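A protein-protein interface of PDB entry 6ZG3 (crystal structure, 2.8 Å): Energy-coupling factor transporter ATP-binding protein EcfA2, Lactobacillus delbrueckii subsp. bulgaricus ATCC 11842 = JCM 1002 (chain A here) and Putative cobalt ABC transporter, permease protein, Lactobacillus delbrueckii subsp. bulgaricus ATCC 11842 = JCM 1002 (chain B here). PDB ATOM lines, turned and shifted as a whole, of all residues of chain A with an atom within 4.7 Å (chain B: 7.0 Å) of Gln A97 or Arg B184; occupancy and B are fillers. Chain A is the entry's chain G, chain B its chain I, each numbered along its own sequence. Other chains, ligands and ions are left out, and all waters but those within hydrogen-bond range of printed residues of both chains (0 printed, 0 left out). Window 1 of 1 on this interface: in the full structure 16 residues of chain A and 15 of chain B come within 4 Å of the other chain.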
ATOM      1  N   PHE A  91     -33.018  16.583  30.054  1.00  0.00           N
ATOM      2  CA  PHE A  91     -34.325  16.779  29.444  1.00  0.00           C
ATOM      3  C   PHE A  91     -34.508  15.808  28.279  1.00  0.00           C
ATOM      4  O   PHE A  91     -33.589  15.079  27.888  1.00  0.00           O
ATOM      5  CB  PHE A  91     -34.494  18.238  29.001  1.00  0.00           C
ATOM      6  CG  PHE A  91     -34.811  19.164  30.131  1.00  0.00           C
ATOM      7  CD1 PHE A  91     -33.918  19.338  31.184  1.00  0.00           C
ATOM      8  CD2 PHE A  91     -36.001  19.838  30.163  1.00  0.00           C
ATOM      9  CE1 PHE A  91     -34.222  20.172  32.245  1.00  0.00           C
ATOM     10  CE2 PHE A  91     -36.308  20.684  31.213  1.00  0.00           C
ATOM     11  CZ  PHE A  91     -35.421  20.851  32.258  1.00  0.00           C
ATOM     12  N   SER A  94     -32.655  15.579  24.307  1.00  0.00           N
ATOM     13  CA  SER A  94     -31.759  16.674  24.632  1.00  0.00           C
ATOM     14  C   SER A  94     -30.755  16.981  23.537  1.00  0.00           C
ATOM     15  O   SER A  94     -30.016  17.947  23.704  1.00  0.00           O
ATOM     16  CB  SER A  94     -31.023  16.377  25.932  1.00  0.00           C
ATOM     17  OG  SER A  94     -30.450  15.098  25.846  1.00  0.00           O
ATOM     18  N   GLU A  95     -30.692  16.231  22.432  1.00  0.00           N
ATOM     19  CA  GLU A  95     -29.834  16.657  21.332  1.00  0.00           C
ATOM     20  C   GLU A  95     -30.151  18.078  20.880  1.00  0.00           C
ATOM     21  O   GLU A  95     -29.331  18.679  20.173  1.00  0.00           O
ATOM     22  CB  GLU A  95     -29.971  15.702  20.146  1.00  0.00           C
ATOM     23  CG  GLU A  95     -31.440  15.383  19.805  1.00  0.00           C
ATOM     24  CD  GLU A  95     -32.020  14.228  20.641  1.00  0.00           C
ATOM     25  OE1 GLU A  95     -31.684  14.131  21.851  1.00  0.00           O
ATOM     26  OE2 GLU A  95     -32.837  13.444  20.102  1.00  0.00           O
ATOM     27  N   ALA A  96     -31.303  18.627  21.294  1.00  0.00           N
ATOM     28  CA  ALA A  96     -31.679  20.005  20.990  1.00  0.00           C
ATOM     29  C   ALA A  96     -30.813  21.029  21.719  1.00  0.00           C
ATOM     30  O   ALA A  96     -30.676  22.163  21.242  1.00  0.00           O
ATOM     31  CB  ALA A  96     -33.157  20.205  21.330  1.00  0.00           C
ATOM     32  N   GLN A  97     -30.205  20.630  22.841  1.00  0.00           N
ATOM     33  CA  GLN A  97     -29.294  21.479  23.612  1.00  0.00           C
ATOM     34  C   GLN A  97     -28.019  21.824  22.839  1.00  0.00           C
ATOM     35  O   GLN A  97     -27.475  22.927  22.993  1.00  0.00           O
ATOM     36  CB  GLN A  97     -28.902  20.755  24.913  1.00  0.00           C
ATOM     37  CG  GLN A  97     -30.049  20.158  25.731  1.00  0.00           C
ATOM     38  CD  GLN A  97     -29.573  19.623  27.054  1.00  0.00           C
ATOM     39  OE1 GLN A  97     -28.425  19.850  27.442  1.00  0.00           O
ATOM     40  NE2 GLN A  97     -30.444  18.908  27.757  1.00  0.00           N
ATOM     41  N   LEU A  98     -27.517  20.880  22.042  1.00  0.00           N
ATOM     42  CA  LEU A  98     -26.253  21.024  21.338  1.00  0.00           C
ATOM     43  C   LEU A  98     -26.199  22.325  20.538  1.00  0.00           C
ATOM     44  O   LEU A  98     -27.149  22.679  19.832  1.00  0.00           O
ATOM     45  CB  LEU A  98     -26.063  19.826  20.406  1.00  0.00           C
ATOM     46  CG  LEU A  98     -25.532  18.514  20.982  1.00  0.00           C
ATOM     47  CD1 LEU A  98     -26.333  18.142  22.178  1.00  0.00           C
ATOM     48  CD2 LEU A  98     -25.554  17.377  19.967  1.00  0.00           C
ATOM     49  N   PHE A  99     -25.071  23.047  20.654  1.00  0.00           N
ATOM     50  CA  PHE A  99     -24.924  24.339  19.981  1.00  0.00           C
ATOM     51  C   PHE A  99     -23.482  24.791  19.704  1.00  0.00           C
ATOM     52  O   PHE A  99     -23.284  25.820  19.056  1.00  0.00           O
ATOM     53  CB  PHE A  99     -25.615  25.429  20.814  1.00  0.00           C
ATOM     54  CG  PHE A  99     -24.847  25.802  22.056  1.00  0.00           C
ATOM     55  CD1 PHE A  99     -24.915  25.012  23.205  1.00  0.00           C
ATOM     56  CD2 PHE A  99     -24.019  26.914  22.067  1.00  0.00           C
ATOM     57  CE1 PHE A  99     -24.187  25.346  24.343  1.00  0.00           C
ATOM     58  CE2 PHE A  99     -23.294  27.236  23.195  1.00  0.00           C
ATOM     59  CZ  PHE A  99     -23.380  26.455  24.326  1.00  0.00           C
ATOM     60  N   ASP A 106     -19.094  21.772  23.216  1.00  0.00           N
ATOM     61  CA  ASP A 106     -20.425  21.707  23.799  1.00  0.00           C
ATOM     62  C   ASP A 106     -20.448  20.808  25.017  1.00  0.00           C
ATOM     63  O   ASP A 106     -21.127  21.124  25.999  1.00  0.00           O
ATOM     64  CB  ASP A 106     -21.447  21.230  22.775  1.00  0.00           C
ATOM     65  CG  ASP A 106     -22.855  21.230  23.331  1.00  0.00           C
ATOM     66  OD1 ASP A 106     -23.524  22.277  23.322  1.00  0.00           O
ATOM     67  OD2 ASP A 106     -23.283  20.167  23.816  1.00  0.00           O
ATOM     68  N   TYR A 109     -19.086  22.652  27.936  1.00  0.00           N
ATOM     69  CA  TYR A 109     -19.929  23.766  28.369  1.00  0.00           C
ATOM     70  C   TYR A 109     -20.367  23.626  29.823  1.00  0.00           C
ATOM     71  O   TYR A 109     -20.224  24.562  30.617  1.00  0.00           O
ATOM     72  CB  TYR A 109     -21.159  23.865  27.456  1.00  0.00           C
ATOM     73  CG  TYR A 109     -22.126  25.011  27.761  1.00  0.00           C
ATOM     74  CD1 TYR A 109     -23.231  24.820  28.592  1.00  0.00           C
ATOM     75  CD2 TYR A 109     -21.918  26.278  27.254  1.00  0.00           C
ATOM     76  CE1 TYR A 109     -24.111  25.853  28.880  1.00  0.00           C
ATOM     77  CE2 TYR A 109     -22.806  27.305  27.520  1.00  0.00           C
ATOM     78  CZ  TYR A 109     -23.898  27.087  28.338  1.00  0.00           C
ATOM     79  OH  TYR A 109     -24.758  28.126  28.610  1.00  0.00           O
ATOM     80  N   GLY A 110     -20.882  22.456  30.199  1.00  0.00           N
ATOM     81  CA  GLY A 110     -21.438  22.265  31.520  1.00  0.00           C
ATOM     82  C   GLY A 110     -20.452  22.529  32.645  1.00  0.00           C
ATOM     83  O   GLY A 110     -20.685  23.374  33.528  1.00  0.00           O
ATOM     84  N   ASN A 113     -19.476  26.235  33.045  1.00  0.00           N
ATOM     85  CA  ASN A 113     -20.465  27.010  33.788  1.00  0.00           C
ATOM     86  C   ASN A 113     -20.452  26.675  35.265  1.00  0.00           C
ATOM     87  O   ASN A 113     -20.811  27.514  36.096  1.00  0.00           O
ATOM     88  CB  ASN A 113     -21.864  26.757  33.243  1.00  0.00           C
ATOM     89  CG  ASN A 113     -22.007  27.185  31.832  1.00  0.00           C
ATOM     90  OD1 ASN A 113     -22.356  28.325  31.568  1.00  0.00           O
ATOM     91  ND2 ASN A 113     -21.733  26.287  30.906  1.00  0.00           N
ATOM     92  N   PHE A 114     -20.056  25.460  35.615  1.00  0.00           N
ATOM     93  CA  PHE A 114     -20.071  25.071  37.012  1.00  0.00           C
ATOM     94  C   PHE A 114     -18.711  25.202  37.663  1.00  0.00           C
ATOM     95  O   PHE A 114     -18.528  24.739  38.792  1.00  0.00           O
ATOM     96  CB  PHE A 114     -20.613  23.653  37.163  1.00  0.00           C
ATOM     97  CG  PHE A 114     -22.096  23.550  36.939  1.00  0.00           C
ATOM     98  CD1 PHE A 114     -22.983  24.239  37.760  1.00  0.00           C
ATOM     99  CD2 PHE A 114     -22.606  22.758  35.934  1.00  0.00           C
ATOM    100  CE1 PHE A 114     -24.351  24.139  37.580  1.00  0.00           C
ATOM    101  CE2 PHE A 114     -23.968  22.654  35.757  1.00  0.00           C
ATOM    102  CZ  PHE A 114     -24.841  23.340  36.585  1.00  0.00           C
ATOM    103  N   ALA A 155     -25.410  15.069  23.904  1.00  0.00           N
ATOM    104  CA  ALA A 155     -26.297  15.752  24.831  1.00  0.00           C
ATOM    105  C   ALA A 155     -26.179  15.179  26.244  1.00  0.00           C
ATOM    106  O   ALA A 155     -26.208  15.933  27.220  1.00  0.00           O
ATOM    107  CB  ALA A 155     -27.731  15.675  24.328  1.00  0.00           C
ATOM    108  N   GLY A 158     -22.660  16.000  28.003  1.00  0.00           N
ATOM    109  CA  GLY A 158     -22.646  17.364  28.501  1.00  0.00           C
ATOM    110  C   GLY A 158     -23.396  17.623  29.793  1.00  0.00           C
ATOM    111  O   GLY A 158     -23.151  18.640  30.452  1.00  0.00           O
ATOM    112  N   VAL A 159     -24.314  16.734  30.170  1.00  0.00           N
ATOM    113  CA  VAL A 159     -25.024  16.894  31.433  1.00  0.00           C
ATOM    114  C   VAL A 159     -24.496  15.959  32.490  1.00  0.00           C
ATOM    115  O   VAL A 159     -24.864  16.107  33.668  1.00  0.00           O
ATOM    116  CB  VAL A 159     -26.547  16.689  31.295  1.00  0.00           C
ATOM    117  CG1 VAL A 159     -27.281  17.680  32.198  1.00  0.00           C
ATOM    118  CG2 VAL A 159     -27.016  16.862  29.861  1.00  0.00           C
ATOM    119  N   TYR A 162     -19.728  16.836  34.409  1.00  0.00           N
ATOM    120  CA  TYR A 162     -19.339  17.411  35.691  1.00  0.00           C
ATOM    121  C   TYR A 162     -19.696  16.500  36.863  1.00  0.00           C
ATOM    122  O   TYR A 162     -19.632  16.932  38.022  1.00  0.00           O
ATOM    123  CB  TYR A 162     -19.981  18.791  35.884  1.00  0.00           C
ATOM    124  CG  TYR A 162     -21.444  18.912  35.535  1.00  0.00           C
ATOM    125  CD1 TYR A 162     -21.867  19.006  34.215  1.00  0.00           C
ATOM    126  CD2 TYR A 162     -22.407  18.949  36.535  1.00  0.00           C
ATOM    127  CE1 TYR A 162     -23.237  19.135  33.892  1.00  0.00           C
ATOM    128  CE2 TYR A 162     -23.774  19.071  36.225  1.00  0.00           C
ATOM    129  CZ  TYR A 162     -24.174  19.162  34.900  1.00  0.00           C
ATOM    130  OH  TYR A 162     -25.499  19.288  34.590  1.00  0.00           O
ATOM    131  N   GLN B 173     -40.786  24.824  22.322  1.00  0.00           N
ATOM    132  CA  GLN B 173     -39.413  24.339  22.175  1.00  0.00           C
ATOM    133  C   GLN B 173     -38.420  25.385  22.654  1.00  0.00           C
ATOM    134  O   GLN B 173     -37.397  25.048  23.269  1.00  0.00           O
ATOM    135  CB  GLN B 173     -39.084  23.949  20.733  1.00  0.00           C
ATOM    136  CG  GLN B 173     -37.723  23.237  20.666  1.00  0.00           C
ATOM    137  CD  GLN B 173     -37.840  21.725  20.934  1.00  0.00           C
ATOM    138  OE1 GLN B 173     -38.871  21.128  20.627  1.00  0.00           O
ATOM    139  NE2 GLN B 173     -36.812  21.120  21.554  1.00  0.00           N
ATOM    140  N   LYS B 176     -38.198  25.046  26.335  1.00  0.00           N
ATOM    141  CA  LYS B 176     -37.554  23.824  26.787  1.00  0.00           C
ATOM    142  C   LYS B 176     -36.045  23.921  26.641  1.00  0.00           C
ATOM    143  O   LYS B 176     -35.301  23.506  27.539  1.00  0.00           O
ATOM    144  CB  LYS B 176     -38.126  22.626  26.035  1.00  0.00           C
ATOM    145  CG  LYS B 176     -39.505  22.233  26.593  1.00  0.00           C
ATOM    146  CD  LYS B 176     -40.305  21.285  25.683  1.00  0.00           C
ATOM    147  CE  LYS B 176     -41.799  21.250  26.035  1.00  0.00           C
ATOM    148  NZ  LYS B 176     -42.583  20.541  24.980  1.00  0.00           N
ATOM    149  N   ILE B 177     -35.573  24.497  25.536  1.00  0.00           N
ATOM    150  CA  ILE B 177     -34.132  24.657  25.379  1.00  0.00           C
ATOM    151  C   ILE B 177     -33.574  25.520  26.496  1.00  0.00           C
ATOM    152  O   ILE B 177     -32.518  25.220  27.067  1.00  0.00           O
ATOM    153  CB  ILE B 177     -33.797  25.233  23.993  1.00  0.00           C
ATOM    154  CG1 ILE B 177     -33.878  24.108  22.962  1.00  0.00           C
ATOM    155  CG2 ILE B 177     -32.418  25.960  23.995  1.00  0.00           C
ATOM    156  CD1 ILE B 177     -33.105  22.867  23.416  1.00  0.00           C
ATOM    157  N   MET B 178     -34.284  26.586  26.845  1.00  0.00           N
ATOM    158  CA  MET B 178     -33.817  27.444  27.921  1.00  0.00           C
ATOM    159  C   MET B 178     -33.685  26.678  29.224  1.00  0.00           C
ATOM    160  O   MET B 178     -32.689  26.817  29.943  1.00  0.00           O
ATOM    161  CB  MET B 178     -34.756  28.625  28.089  1.00  0.00           C
ATOM    162  CG  MET B 178     -34.511  29.724  27.080  1.00  0.00           C
ATOM    163  SD  MET B 178     -35.220  31.262  27.688  1.00  0.00           S
ATOM    164  CE  MET B 178     -36.900  30.733  28.082  1.00  0.00           C
ATOM    165  N   ASN B 179     -34.683  25.863  29.551  1.00  0.00           N
ATOM    166  CA  ASN B 179     -34.593  25.114  30.802  1.00  0.00           C
ATOM    167  C   ASN B 179     -33.478  24.071  30.766  1.00  0.00           C
ATOM    168  O   ASN B 179     -32.784  23.856  31.771  1.00  0.00           O
ATOM    169  CB  ASN B 179     -35.939  24.493  31.123  1.00  0.00           C
ATOM    170  CG  ASN B 179     -36.920  25.515  31.621  1.00  0.00           C
ATOM    171  OD1 ASN B 179     -36.532  26.520  32.231  1.00  0.00           O
ATOM    172  ND2 ASN B 179     -38.196  25.282  31.362  1.00  0.00           N
ATOM    173  N   ALA B 180     -33.293  23.410  29.626  1.00  0.00           N
ATOM    174  CA  ALA B 180     -32.192  22.464  29.507  1.00  0.00           C
ATOM    175  C   ALA B 180     -30.859  23.156  29.774  1.00  0.00           C
ATOM    176  O   ALA B 180     -30.033  22.674  30.566  1.00  0.00           O
ATOM    177  CB  ALA B 180     -32.220  21.803  28.135  1.00  0.00           C
ATOM    178  N   GLN B 181     -30.648  24.324  29.157  1.00  0.00           N
ATOM    179  CA  GLN B 181     -29.374  25.011  29.347  1.00  0.00           C
ATOM    180  C   GLN B 181     -29.224  25.536  30.771  1.00  0.00           C
ATOM    181  O   GLN B 181     -28.133  25.482  31.340  1.00  0.00           O
ATOM    182  CB  GLN B 181     -29.191  26.131  28.329  1.00  0.00           C
ATOM    183  CG  GLN B 181     -29.459  25.750  26.877  1.00  0.00           C
ATOM    184  CD  GLN B 181     -28.572  24.651  26.330  1.00  0.00           C
ATOM    185  OE1 GLN B 181     -28.164  23.752  27.045  1.00  0.00           O
ATOM    186  NE2 GLN B 181     -28.258  24.732  25.047  1.00  0.00           N
ATOM    187  N   ARG B 182     -30.294  26.027  31.384  1.00  0.00           N
ATOM    188  CA  ARG B 182     -30.178  26.371  32.797  1.00  0.00           C
ATOM    189  C   ARG B 182     -29.800  25.155  33.628  1.00  0.00           C
ATOM    190  O   ARG B 182     -29.087  25.284  34.629  1.00  0.00           O
ATOM    191  CB  ARG B 182     -31.487  26.947  33.307  1.00  0.00           C
ATOM    192  CG  ARG B 182     -31.965  28.137  32.508  1.00  0.00           C
ATOM    193  CD  ARG B 182     -33.295  28.684  33.024  1.00  0.00           C
ATOM    194  NE  ARG B 182     -33.450  30.096  32.673  1.00  0.00           N
ATOM    195  CZ  ARG B 182     -34.015  31.003  33.465  1.00  0.00           C
ATOM    196  NH1 ARG B 182     -34.473  30.650  34.663  1.00  0.00           N
ATOM    197  NH2 ARG B 182     -34.099  32.267  33.070  1.00  0.00           N
ATOM    198  N   SER B 183     -30.253  23.969  33.212  1.00  0.00           N
ATOM    199  CA  SER B 183     -29.955  22.749  33.951  1.00  0.00           C
ATOM    200  C   SER B 183     -28.494  22.349  33.791  1.00  0.00           C
ATOM    201  O   SER B 183     -27.936  21.670  34.667  1.00  0.00           O
ATOM    202  CB  SER B 183     -30.893  21.645  33.488  1.00  0.00           C
ATOM    203  OG  SER B 183     -32.242  22.048  33.669  1.00  0.00           O
ATOM    204  N   ARG B 184     -27.873  22.741  32.675  1.00  0.00           N
ATOM    205  CA  ARG B 184     -26.419  22.699  32.575  1.00  0.00           C
ATOM    206  C   ARG B 184     -25.780  23.834  33.333  1.00  0.00           C
ATOM    207  O   ARG B 184     -24.576  24.040  33.187  1.00  0.00           O
ATOM    208  CB  ARG B 184     -25.918  22.827  31.141  1.00  0.00           C
ATOM    209  CG  ARG B 184     -26.167  21.680  30.232  1.00  0.00           C
ATOM    210  CD  ARG B 184     -26.252  22.179  28.815  1.00  0.00           C
ATOM    211  NE  ARG B 184     -25.052  21.913  28.045  1.00  0.00           N
ATOM    212  CZ  ARG B 184     -25.026  21.943  26.721  1.00  0.00           C
ATOM    213  NH1 ARG B 184     -26.124  22.223  26.055  1.00  0.00           N
ATOM    214  NH2 ARG B 184     -23.910  21.686  26.065  1.00  0.00           N
ATOM    215  N   GLY B 185     -26.564  24.635  34.047  1.00  0.00           N
ATOM    216  CA  GLY B 185     -26.001  25.760  34.768  1.00  0.00           C
ATOM    217  C   GLY B 185     -25.770  27.010  33.953  1.00  0.00           C
ATOM    218  O   GLY B 185     -24.833  27.759  34.247  1.00  0.00           O
ATOM    219  N   ALA B 186     -26.567  27.242  32.917  1.00  0.00           N
ATOM    220  CA  ALA B 186     -26.447  28.471  32.163  1.00  0.00           C
ATOM    221  C   ALA B 186     -27.242  29.565  32.850  1.00  0.00           C
ATOM    222  O   ALA B 186     -28.283  29.321  33.465  1.00  0.00           O
ATOM    223  CB  ALA B 186     -26.931  28.303  30.731  1.00  0.00           C
ATOM    224  N   VAL B 201     -26.429  32.502  22.596  1.00  0.00           N
ATOM    225  CA  VAL B 201     -26.095  31.460  21.614  1.00  0.00           C
ATOM    226  C   VAL B 201     -26.600  30.092  22.046  1.00  0.00           C
ATOM    227  O   VAL B 201     -27.112  29.342  21.191  1.00  0.00           O
ATOM    228  CB  VAL B 201     -24.589  31.481  21.319  1.00  0.00           C
ATOM    229  CG1 VAL B 201     -24.299  30.756  20.032  1.00  0.00           C
ATOM    230  CG2 VAL B 201     -24.066  32.934  21.262  1.00  0.00           C
ATOM    231  N   PRO B 202     -26.460  29.683  23.314  1.00  0.00           N
ATOM    232  CA  PRO B 202     -27.079  28.429  23.778  1.00  0.00           C
ATOM    233  C   PRO B 202     -28.593  28.400  23.683  1.00  0.00           C
ATOM    234  O   PRO B 202     -29.184  27.375  24.046  1.00  0.00           O
ATOM    235  CB  PRO B 202     -26.628  28.334  25.235  1.00  0.00           C
ATOM    236  CG  PRO B 202     -25.353  29.081  25.272  1.00  0.00           C
ATOM    237  CD  PRO B 202     -25.573  30.243  24.350  1.00  0.00           C
ATOM    238  N   MET B 203     -29.250  29.500  23.311  1.00  0.00           N
ATOM    239  CA  MET B 203     -30.664  29.437  22.968  1.00  0.00           C
ATOM    240  C   MET B 203     -30.931  29.669  21.484  1.00  0.00           C
ATOM    241  O   MET B 203     -31.854  29.073  20.926  1.00  0.00           O
ATOM    242  CB  MET B 203     -31.460  30.444  23.808  1.00  0.00           C
ATOM    243  CG  MET B 203     -32.754  30.876  23.163  1.00  0.00           C
ATOM    244  SD  MET B 203     -33.666  32.067  24.140  1.00  0.00           S
ATOM    245  CE  MET B 203     -33.861  33.409  22.962  1.00  0.00           C
ATOM    246  N   VAL B 205     -28.793  29.008  18.637  1.00  0.00           N
ATOM    247  CA  VAL B 205     -28.415  27.918  17.726  1.00  0.00           C
ATOM    248  C   VAL B 205     -29.400  26.762  17.850  1.00  0.00           C
ATOM    249  O   VAL B 205     -29.862  26.257  16.809  1.00  0.00           O
ATOM    250  CB  VAL B 205     -26.949  27.517  17.942  1.00  0.00           C
ATOM    251  CG1 VAL B 205     -26.481  26.639  16.812  1.00  0.00           C
ATOM    252  CG2 VAL B 205     -26.111  28.702  17.948  1.00  0.00           C
ATOM    253  N   PRO B 206     -29.832  26.344  19.051  1.00  0.00           N
ATOM    254  CA  PRO B 206     -30.884  25.332  19.110  1.00  0.00           C
ATOM    255  C   PRO B 206     -32.132  25.688  18.327  1.00  0.00           C
ATOM    256  O   PRO B 206     -32.620  24.856  17.559  1.00  0.00           O
ATOM    257  CB  PRO B 206     -31.171  25.244  20.615  1.00  0.00           C
ATOM    258  CG  PRO B 206     -29.913  25.511  21.219  1.00  0.00           C
ATOM    259  CD  PRO B 206     -29.299  26.602  20.398  1.00  0.00           C
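NE2 of Gln B181 is in hydrogen-bond range of O of Gln A97 (2.8 Å). The backbone carbonyl oxygen of Gln A97 lies close to the guanidinium group of Arg B184 (3.4 Å). NH2 of Arg B184 is in salt-bridge range of OD2 of Asp A106, 2.8 Å away. The side-chain hydroxyl (OH) of Tyr A162 sits at hydrogen-bond distance from the backbone carbonyl oxygen (O) of Ser B183.
The backbone NH of Phe A99 lies close to the side-chain carboxylate of Asp A106 (3.2 Å). The backbone carbonyl oxygen of Val A159 sits close to the side-chain hydroxyl of Tyr A162, 3.4 Å away. OG of Ser B183 is in hydrogen-bond range of O of Asn B179, at 2.7 Å. The side-chain amide oxygen (OE1) of Gln B181 is in hydrogen-bond range of the guanidinium group (NH1) of Arg B184. N of Ala B186 is in hydrogen-bond range of O of Gln B181 (2.8 Å). The backbone carbonyl oxygen (O) of Pro B202 lies within hydrogen-bond range of the side-chain amide nitrogen (NE2) of Gln B181 (3.0 Å).
Phe A91 touches Asn B179. CE1 of Phe A91 touches OG of Ser B183 (3.1 Å). Ala A96 touches Gln B173 (CB to NE2, 3.8 Å). Ala A96 touches Ile B177. Ala A96 touches Pro B206 (O to CB, 3.2 Å). Gln A97 touches Ile B177 (N to CD1, 3.7 Å). CZ of Phe A99 touches CG of Pro B202, 3.4 Å away. Phe A99 touches Val B205 (CB to CB, 3.8 Å). CG of Pro B202 touches OH of Tyr A109 (3.5 Å). O of Gly B185 touches CB of Asn A113, 3.3 Å away.
Of chain B, only Ile B177 (3.7 Å), Ala B180 (3.4 Å), Gln B181 (2.8 Å), Arg B184 (3.3 Å) and Pro B206 (3.97 Å) come within 4 Å of Gln A97. Printed residues of chain B within 4 Å of Phe A99: Gln B181 (3.8 Å), Pro B202 (3.4 Å), Val B205 (3.8 Å) and Pro B206 (3.9 Å). Of the printed residues of chain B, Tyr A109 touches Arg B184 (3.5 Å), Ala B186 (3.0 Å) and Pro B202 (3.5 Å). Of the printed residues of chain A, Ile B177 touches Ala A96 (3.3 Å) and Gln A97 (3.7 Å). Printed residues of chain A within 4 Å of Ser B183: Phe A91 and Tyr A162. Arg B184 touches just these residues of chain A: Gln A97, Asp A106, Tyr A109, Gly A110, Asn A113 and Phe A114. Of the printed residues of chain A, Ala B186 touches Tyr A109. The nearest residue of chain B that does not touch Gln A97 is Pro B202 (4.9 Å). The nearest printed residue of chain A that does not touch Gln B173 is Gln A97 (6.7 Å).
Of the 17 printed residues of chain B, 12 touch a printed residue of chain A. Hydrophobic or aromatic side chains of chain B that line the printed part of chain A: Ile B177, Ala B180, Ala B186, Pro B202, Val B205 and Pro B206. Among the printed residues, Asp or Glu carboxylates within 4 Å of a Lys or Arg side-chain nitrogen of the other chain: Asp A106 with Arg B184 (2.8 Å).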
